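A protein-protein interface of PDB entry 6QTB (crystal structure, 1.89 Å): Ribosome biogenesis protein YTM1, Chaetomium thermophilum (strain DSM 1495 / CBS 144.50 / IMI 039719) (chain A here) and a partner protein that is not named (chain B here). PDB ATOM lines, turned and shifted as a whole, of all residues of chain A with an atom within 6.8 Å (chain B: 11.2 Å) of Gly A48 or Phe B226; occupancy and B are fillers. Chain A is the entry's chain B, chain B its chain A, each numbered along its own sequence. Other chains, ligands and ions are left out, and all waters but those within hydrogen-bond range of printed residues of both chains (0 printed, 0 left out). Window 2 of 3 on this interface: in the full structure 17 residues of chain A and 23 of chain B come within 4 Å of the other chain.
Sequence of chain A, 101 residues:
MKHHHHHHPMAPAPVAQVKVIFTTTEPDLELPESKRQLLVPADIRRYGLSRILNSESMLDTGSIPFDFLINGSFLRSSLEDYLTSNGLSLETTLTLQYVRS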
ATOM      1  N   VAL A  40     -22.212 -15.620   8.796  1.00  0.00           N
ATOM      2  CA  VAL A  40     -21.294 -14.780   8.024  1.00  0.00           C
ATOM      3  C   VAL A  40     -20.266 -15.668   7.335  1.00  0.00           C
ATOM      4  O   VAL A  40     -19.968 -16.782   7.808  1.00  0.00           O
ATOM      5  CB  VAL A  40     -20.621 -13.709   8.922  1.00  0.00           C
ATOM      6  CG1 VAL A  40     -21.764 -12.809   9.567  1.00  0.00           C
ATOM      7  CG2 VAL A  40     -19.753 -14.324   9.988  1.00  0.00           C
ATOM      8  N   PRO A  41     -19.709 -15.209   6.212  1.00  0.00           N
ATOM      9  CA  PRO A  41     -18.618 -15.960   5.566  1.00  0.00           C
ATOM     10  C   PRO A  41     -17.463 -16.193   6.535  1.00  0.00           C
ATOM     11  O   PRO A  41     -17.038 -15.292   7.261  1.00  0.00           O
ATOM     12  CB  PRO A  41     -18.184 -15.048   4.408  1.00  0.00           C
ATOM     13  CG  PRO A  41     -19.254 -14.055   4.223  1.00  0.00           C
ATOM     14  CD  PRO A  41     -20.004 -13.935   5.531  1.00  0.00           C
ATOM     15  N   ILE A  44     -14.283 -13.973   6.852  1.00  0.00           N
ATOM     16  CA  ILE A  44     -14.418 -12.545   7.186  1.00  0.00           C
ATOM     17  C   ILE A  44     -13.480 -12.176   8.334  1.00  0.00           C
ATOM     18  O   ILE A  44     -13.164 -13.003   9.207  1.00  0.00           O
ATOM     19  CB  ILE A  44     -15.900 -12.237   7.511  1.00  0.00           C
ATOM     20  CG1 ILE A  44     -16.181 -10.738   7.392  1.00  0.00           C
ATOM     21  CG2 ILE A  44     -16.283 -12.787   8.922  1.00  0.00           C
ATOM     22  CD1 ILE A  44     -17.676 -10.457   7.335  1.00  0.00           C
ATOM     23  N   ARG A  45     -13.003 -10.930   8.324  1.00  0.00           N
ATOM     24  CA  ARG A  45     -12.180 -10.325   9.379  1.00  0.00           C
ATOM     25  C   ARG A  45     -12.938  -9.164   9.992  1.00  0.00           C
ATOM     26  O   ARG A  45     -14.068  -8.875   9.595  1.00  0.00           O
ATOM     27  CB  ARG A  45     -10.847  -9.817   8.794  1.00  0.00           C
ATOM     28  CG  ARG A  45     -10.150 -10.916   8.017  1.00  0.00           C
ATOM     29  CD  ARG A  45      -8.836 -10.381   7.339  1.00  0.00           C
ATOM     30  NE  ARG A  45      -7.991  -9.971   8.412  1.00  0.00           N
ATOM     31  CZ  ARG A  45      -6.962 -10.676   8.864  1.00  0.00           C
ATOM     32  NH1 ARG A  45      -6.646 -11.813   8.294  1.00  0.00           N
ATOM     33  NH2 ARG A  45      -6.272 -10.244   9.903  1.00  0.00           N
ATOM     34  N   ARG A  46     -12.304  -8.475  10.964  1.00  0.00           N
ATOM     35  CA  ARG A  46     -13.016  -7.369  11.618  1.00  0.00           C
ATOM     36  C   ARG A  46     -13.460  -6.289  10.622  1.00  0.00           C
ATOM     37  O   ARG A  46     -14.469  -5.642  10.830  1.00  0.00           O
ATOM     38  CB  ARG A  46     -12.141  -6.780  12.742  1.00  0.00           C
ATOM     39  CG  ARG A  46     -10.883  -6.056  12.264  1.00  0.00           C
ATOM     40  CD  ARG A  46     -10.657  -4.741  13.112  1.00  0.00           C
ATOM     41  NE  ARG A  46     -11.782  -3.830  12.946  1.00  0.00           N
ATOM     42  CZ  ARG A  46     -11.923  -3.025  11.885  1.00  0.00           C
ATOM     43  NH1 ARG A  46     -12.954  -2.204  11.819  1.00  0.00           N
ATOM     44  NH2 ARG A  46     -11.012  -3.039  10.863  1.00  0.00           N
ATOM     45  N   TYR A  47     -12.663  -6.015   9.579  1.00  0.00           N
ATOM     46  CA  TYR A  47     -13.037  -4.996   8.587  1.00  0.00           C
ATOM     47  C   TYR A  47     -14.411  -5.271   7.984  1.00  0.00           C
ATOM     48  O   TYR A  47     -15.319  -4.409   7.996  1.00  0.00           O
ATOM     49  CB  TYR A  47     -11.967  -4.980   7.477  1.00  0.00           C
ATOM     50  CG  TYR A  47     -12.169  -3.910   6.448  1.00  0.00           C
ATOM     51  CD1 TYR A  47     -11.663  -2.621   6.681  1.00  0.00           C
ATOM     52  CD2 TYR A  47     -12.762  -4.174   5.209  1.00  0.00           C
ATOM     53  CE1 TYR A  47     -11.796  -1.617   5.772  1.00  0.00           C
ATOM     54  CE2 TYR A  47     -12.907  -3.096   4.242  1.00  0.00           C
ATOM     55  CZ  TYR A  47     -12.411  -1.848   4.567  1.00  0.00           C
ATOM     56  OH  TYR A  47     -12.468  -0.773   3.698  1.00  0.00           O
ATOM     57  N   GLY A  48     -14.593  -6.489   7.483  1.00  0.00           N
ATOM     58  CA  GLY A  48     -15.895  -6.904   6.957  1.00  0.00           C
ATOM     59  C   GLY A  48     -17.012  -6.965   7.998  1.00  0.00           C
ATOM     60  O   GLY A  48     -18.157  -6.622   7.690  1.00  0.00           O
ATOM     61  N   LEU A  49     -16.718  -7.463   9.220  1.00  0.00           N
ATOM     62  CA  LEU A  49     -17.767  -7.465  10.256  1.00  0.00           C
ATOM     63  C   LEU A  49     -18.224  -6.042  10.551  1.00  0.00           C
ATOM     64  O   LEU A  49     -19.411  -5.801  10.791  1.00  0.00           O
ATOM     65  CB  LEU A  49     -17.262  -8.168  11.539  1.00  0.00           C
ATOM     66  CG  LEU A  49     -16.987  -9.692  11.336  1.00  0.00           C
ATOM     67  CD1 LEU A  49     -15.998 -10.274  12.339  1.00  0.00           C
ATOM     68  CD2 LEU A  49     -18.340 -10.468  11.410  1.00  0.00           C
ATOM     69  N   SER A  50     -17.297  -5.074  10.567  1.00  0.00           N
ATOM     70  CA  SER A  50     -17.689  -3.683  10.853  1.00  0.00           C
ATOM     71  C   SER A  50     -18.594  -3.138   9.755  1.00  0.00           C
ATOM     72  O   SER A  50     -19.567  -2.412  10.030  1.00  0.00           O
ATOM     73  CB  SER A  50     -16.419  -2.827  11.025  1.00  0.00           C
ATOM     74  OG  SER A  50     -16.715  -1.484  11.370  1.00  0.00           O
ATOM     75  N   ARG A  51     -18.293  -3.478   8.489  1.00  0.00           N
ATOM     76  CA  ARG A  51     -19.170  -3.062   7.389  1.00  0.00           C
ATOM     77  C   ARG A  51     -20.567  -3.630   7.519  1.00  0.00           C
ATOM     78  O   ARG A  51     -21.545  -2.942   7.213  1.00  0.00           O
ATOM     79  CB  ARG A  51     -18.551  -3.466   6.065  1.00  0.00           C
ATOM     80  CG  ARG A  51     -17.158  -2.771   5.954  1.00  0.00           C
ATOM     81  CD  ARG A  51     -17.170  -1.171   6.023  1.00  0.00           C
ATOM     82  NE  ARG A  51     -17.353  -0.461   7.319  1.00  0.00           N
ATOM     83  CZ  ARG A  51     -16.566  -0.533   8.403  1.00  0.00           C
ATOM     84  NH1 ARG A  51     -15.490  -1.262   8.421  1.00  0.00           N
ATOM     85  NH2 ARG A  51     -16.848   0.144   9.506  1.00  0.00           N
ATOM     86  N   ILE A  52     -20.676  -4.905   7.907  1.00  0.00           N
ATOM     87  CA  ILE A  52     -22.003  -5.495   8.142  1.00  0.00           C
ATOM     88  C   ILE A  52     -22.757  -4.711   9.206  1.00  0.00           C
ATOM     89  O   ILE A  52     -23.949  -4.336   9.026  1.00  0.00           O
ATOM     90  CB  ILE A  52     -21.842  -6.975   8.542  1.00  0.00           C
ATOM     91  CG1 ILE A  52     -21.451  -7.817   7.319  1.00  0.00           C
ATOM     92  CG2 ILE A  52     -23.134  -7.532   9.161  1.00  0.00           C
ATOM     93  CD1 ILE A  52     -21.082  -9.283   7.677  1.00  0.00           C
ATOM     94  N   LEU A  53     -22.095  -4.460  10.353  1.00  0.00           N
ATOM     95  CA  LEU A  53     -22.784  -3.775  11.462  1.00  0.00           C
ATOM     96  C   LEU A  53     -23.264  -2.387  11.053  1.00  0.00           C
ATOM     97  O   LEU A  53     -24.333  -1.919  11.507  1.00  0.00           O
ATOM     98  CB  LEU A  53     -21.856  -3.619  12.649  1.00  0.00           C
ATOM     99  CG  LEU A  53     -21.757  -4.689  13.721  1.00  0.00           C
ATOM    100  CD1 LEU A  53     -20.935  -4.109  14.916  1.00  0.00           C
ATOM    101  CD2 LEU A  53     -23.209  -5.119  14.154  1.00  0.00           C
ATOM    102  N   PHE A  68     -13.872  -6.015  17.719  1.00  0.00           N
ATOM    103  CA  PHE A  68     -14.691  -7.116  18.233  1.00  0.00           C
ATOM    104  C   PHE A  68     -13.901  -7.909  19.275  1.00  0.00           C
ATOM    105  O   PHE A  68     -12.721  -8.236  19.059  1.00  0.00           O
ATOM    106  CB  PHE A  68     -15.158  -8.035  17.086  1.00  0.00           C
ATOM    107  CG  PHE A  68     -15.950  -7.309  16.023  1.00  0.00           C
ATOM    108  CD1 PHE A  68     -15.302  -6.648  14.970  1.00  0.00           C
ATOM    109  CD2 PHE A  68     -17.327  -7.230  16.113  1.00  0.00           C
ATOM    110  CE1 PHE A  68     -16.032  -5.925  14.008  1.00  0.00           C
ATOM    111  CE2 PHE A  68     -18.080  -6.529  15.150  1.00  0.00           C
ATOM    112  CZ  PHE A  68     -17.442  -5.864  14.093  1.00  0.00           C
ATOM    113  N   GLU B 223     -28.673 -14.306   7.575  1.00  0.00           N
ATOM    114  CA  GLU B 223     -27.373 -14.586   6.982  1.00  0.00           C
ATOM    115  C   GLU B 223     -26.929 -13.442   6.084  1.00  0.00           C
ATOM    116  O   GLU B 223     -27.729 -12.901   5.320  1.00  0.00           O
ATOM    117  CB  GLU B 223     -27.360 -15.857   6.148  1.00  0.00           C
ATOM    118  CG  GLU B 223     -28.398 -16.009   5.153  1.00  0.00           C
ATOM    119  CD  GLU B 223     -28.157 -17.297   4.373  1.00  0.00           C
ATOM    120  OE1 GLU B 223     -27.063 -17.443   3.761  1.00  0.00           O
ATOM    121  OE2 GLU B 223     -29.005 -18.201   4.460  1.00  0.00           O
ATOM    122  N   ALA B 224     -25.640 -13.106   6.168  1.00  0.00           N
ATOM    123  CA  ALA B 224     -25.037 -12.014   5.403  1.00  0.00           C
ATOM    124  C   ALA B 224     -24.259 -12.573   4.214  1.00  0.00           C
ATOM    125  O   ALA B 224     -23.426 -13.476   4.376  1.00  0.00           O
ATOM    126  CB  ALA B 224     -24.102 -11.169   6.276  1.00  0.00           C
ATOM    127  N   ARG B 225     -24.522 -12.014   3.041  1.00  0.00           N
ATOM    128  CA  ARG B 225     -23.788 -12.284   1.814  1.00  0.00           C
ATOM    129  C   ARG B 225     -23.258 -10.959   1.282  1.00  0.00           C
ATOM    130  O   ARG B 225     -23.943  -9.938   1.380  1.00  0.00           O
ATOM    131  CB  ARG B 225     -24.716 -12.932   0.784  1.00  0.00           C
ATOM    132  CG  ARG B 225     -25.475 -14.156   1.310  1.00  0.00           C
ATOM    133  CD  ARG B 225     -26.279 -14.799   0.190  1.00  0.00           C
ATOM    134  NE  ARG B 225     -26.932 -16.032   0.604  1.00  0.00           N
ATOM    135  CZ  ARG B 225     -26.354 -17.222   0.523  1.00  0.00           C
ATOM    136  NH1 ARG B 225     -25.121 -17.318   0.032  1.00  0.00           N
ATOM    137  NH2 ARG B 225     -27.005 -18.312   0.919  1.00  0.00           N
ATOM    138  N   PHE B 226     -22.042 -10.951   0.747  1.00  0.00           N
ATOM    139  CA  PHE B 226     -21.541  -9.736   0.116  1.00  0.00           C
ATOM    140  C   PHE B 226     -21.830  -9.807  -1.379  1.00  0.00           C
ATOM    141  O   PHE B 226     -21.480 -10.793  -2.035  1.00  0.00           O
ATOM    142  CB  PHE B 226     -20.047  -9.569   0.355  1.00  0.00           C
ATOM    143  CG  PHE B 226     -19.698  -9.127   1.741  1.00  0.00           C
ATOM    144  CD1 PHE B 226     -19.791  -7.805   2.103  1.00  0.00           C
ATOM    145  CD2 PHE B 226     -19.278 -10.060   2.698  1.00  0.00           C
ATOM    146  CE1 PHE B 226     -19.439  -7.394   3.414  1.00  0.00           C
ATOM    147  CE2 PHE B 226     -18.944  -9.655   3.999  1.00  0.00           C
ATOM    148  CZ  PHE B 226     -19.013  -8.309   4.346  1.00  0.00           C
ATOM    149  N   GLY B 227     -22.480  -8.766  -1.899  1.00  0.00           N
ATOM    150  CA  GLY B 227     -22.846  -8.656  -3.293  1.00  0.00           C
ATOM    151  C   GLY B 227     -21.686  -8.333  -4.222  1.00  0.00           C
ATOM    152  O   GLY B 227     -20.554  -8.070  -3.792  1.00  0.00           O
ATOM    153  N   PRO B 228     -21.951  -8.360  -5.536  1.00  0.00           N
ATOM    154  CA  PRO B 228     -20.875  -8.045  -6.494  1.00  0.00           C
ATOM    155  C   PRO B 228     -20.272  -6.670  -6.274  1.00  0.00           C
ATOM    156  O   PRO B 228     -19.066  -6.496  -6.467  1.00  0.00           O
ATOM    157  CB  PRO B 228     -21.579  -8.134  -7.867  1.00  0.00           C
ATOM    158  CG  PRO B 228     -22.940  -8.795  -7.604  1.00  0.00           C
ATOM    159  CD  PRO B 228     -23.277  -8.502  -6.179  1.00  0.00           C
ATOM    160  N   ASP B 229     -21.095  -5.681  -5.903  1.00  0.00           N
ATOM    161  CA  ASP B 229     -20.689  -4.341  -5.472  1.00  0.00           C
ATOM    162  C   ASP B 229     -19.965  -4.313  -4.126  1.00  0.00           C
ATOM    163  O   ASP B 229     -19.494  -3.240  -3.736  1.00  0.00           O
ATOM    164  CB  ASP B 229     -21.897  -3.409  -5.426  1.00  0.00           C
ATOM    165  CG  ASP B 229     -23.049  -3.971  -4.622  1.00  0.00           C
ATOM    166  OD1 ASP B 229     -23.132  -5.205  -4.439  1.00  0.00           O
ATOM    167  OD2 ASP B 229     -23.939  -3.160  -4.270  1.00  0.00           O
ATOM    168  N   GLY B 230     -20.000  -5.406  -3.345  1.00  0.00           N
ATOM    169  CA  GLY B 230     -19.397  -5.462  -2.023  1.00  0.00           C
ATOM    170  C   GLY B 230     -20.322  -5.069  -0.882  1.00  0.00           C
ATOM    171  O   GLY B 230     -19.890  -5.053   0.270  1.00  0.00           O
ATOM    172  N   VAL B 231     -21.571  -4.752  -1.158  1.00  0.00           N
ATOM    173  CA  VAL B 231     -22.456  -4.265  -0.110  1.00  0.00           C
ATOM    174  C   VAL B 231     -23.038  -5.515   0.555  1.00  0.00           C
ATOM    175  O   VAL B 231     -23.391  -6.480  -0.146  1.00  0.00           O
ATOM    176  CB  VAL B 231     -23.521  -3.328  -0.698  1.00  0.00           C
ATOM    177  CG1 VAL B 231     -24.549  -2.932   0.337  1.00  0.00           C
ATOM    178  CG2 VAL B 231     -22.848  -2.094  -1.364  1.00  0.00           C
ATOM    179  N   PRO B 232     -23.108  -5.587   1.883  1.00  0.00           N
ATOM    180  CA  PRO B 232     -23.675  -6.796   2.502  1.00  0.00           C
ATOM    181  C   PRO B 232     -25.168  -6.827   2.258  1.00  0.00           C
ATOM    182  O   PRO B 232     -25.831  -5.789   2.263  1.00  0.00           O
ATOM    183  CB  PRO B 232     -23.363  -6.629   3.995  1.00  0.00           C
ATOM    184  CG  PRO B 232     -22.594  -5.338   4.154  1.00  0.00           C
ATOM    185  CD  PRO B 232     -22.801  -4.545   2.889  1.00  0.00           C
ATOM    186  N   VAL B 233     -25.691  -8.004   1.926  1.00  0.00           N
ATOM    187  CA  VAL B 233     -27.135  -8.184   1.864  1.00  0.00           C
ATOM    188  C   VAL B 233     -27.525  -9.301   2.825  1.00  0.00           C
ATOM    189  O   VAL B 233     -26.829 -10.317   2.942  1.00  0.00           O
ATOM    190  CB  VAL B 233     -27.641  -8.435   0.428  1.00  0.00           C
ATOM    191  CG1 VAL B 233     -27.634  -7.098  -0.342  1.00  0.00           C
ATOM    192  CG2 VAL B 233     -26.757  -9.413  -0.293  1.00  0.00           C
ATOM    193  N   ILE B 234     -28.612  -9.077   3.549  1.00  0.00           N
ATOM    194  CA  ILE B 234     -28.994  -9.943   4.660  1.00  0.00           C
ATOM    195  C   ILE B 234     -30.373 -10.527   4.390  1.00  0.00           C
ATOM    196  O   ILE B 234     -31.305  -9.793   4.055  1.00  0.00           O
ATOM    197  CB  ILE B 234     -28.930  -9.157   5.967  1.00  0.00           C
ATOM    198  CG1 ILE B 234     -27.458  -8.733   6.166  1.00  0.00           C
ATOM    199  CG2 ILE B 234     -29.438  -9.996   7.134  1.00  0.00           C
ATOM    200  CD1 ILE B 234     -27.268  -7.845   7.334  1.00  0.00           C
ATOM    201  N   HIS B 235     -30.498 -11.845   4.564  1.00  0.00           N
ATOM    202  CA  HIS B 235     -31.683 -12.642   4.279  1.00  0.00           C
ATOM    203  C   HIS B 235     -31.991 -13.461   5.529  1.00  0.00           C
ATOM    204  O   HIS B 235     -31.084 -13.701   6.318  1.00  0.00           O
ATOM    205  CB  HIS B 235     -31.425 -13.685   3.170  1.00  0.00           C
ATOM    206  CG  HIS B 235     -30.890 -13.132   1.893  1.00  0.00           C
ATOM    207  ND1 HIS B 235     -31.702 -12.623   0.903  1.00  0.00           N
ATOM    208  CD2 HIS B 235     -29.626 -13.059   1.417  1.00  0.00           C
ATOM    209  CE1 HIS B 235     -30.963 -12.239  -0.120  1.00  0.00           C
ATOM    210  NE2 HIS B 235     -29.699 -12.486   0.168  1.00  0.00           N
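Of the printed residues of chain B, Pro A41 touches Ala B224.
Ile A44 touches one residue of chain B.
Arg A46 touches none of the printed residues of chain B.
Of chain B, only Phe B226 (3.8 Å) comes within 4 Å of Gly A48.
Ser A50 touches none of the printed residues of chain B.
Of the printed residues of chain B, Ile A52 touches Ala B224 (3.8 Å) and Phe B226 (3.9 Å).
Of the printed residues of chain A, Ala B224 touches Pro A41 (3.6 Å) and Ile A52 (3.8 Å).
Of chain A, only Ile A44 (3.7 Å), Gly A48 (3.8 Å) and Ile A52 (3.9 Å) come within 4 Å of Phe B226.
The nearest residue of chain A that does not touch Phe B226 is Pro A41 (4.3 Å).
Pro A41 touches Ala B224 (CD to O, 3.6 Å).
Phe B226 touches Ile A44 (CE2 to CD1, 3.7 Å).
CZ of Phe B226 touches O of Gly A48 (3.8 Å).
Ile A52 touches Ala B224 (CD1 to CB, 3.8 Å).
Ile A52 touches Phe B226 (CG1 to CZ, 3.9 Å).
Of the 13 printed residues of chain A, 4 touch a printed residue of chain B.
Hydrophobic or aromatic side chains of chain A within 4 Å of the printed part of chain B: Pro A41, Ile A44 and Ile A52.
Hydrophobic or aromatic side chains of chain B within 4 Å of the printed part of chain A: Ala B224 and Phe B226.
Among the printed residues, 5 pairs touch across the chains.
Among the printed residues, no Asp or Glu carboxylate lies within 4 Å of a Lys or Arg side-chain nitrogen of the other chain.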
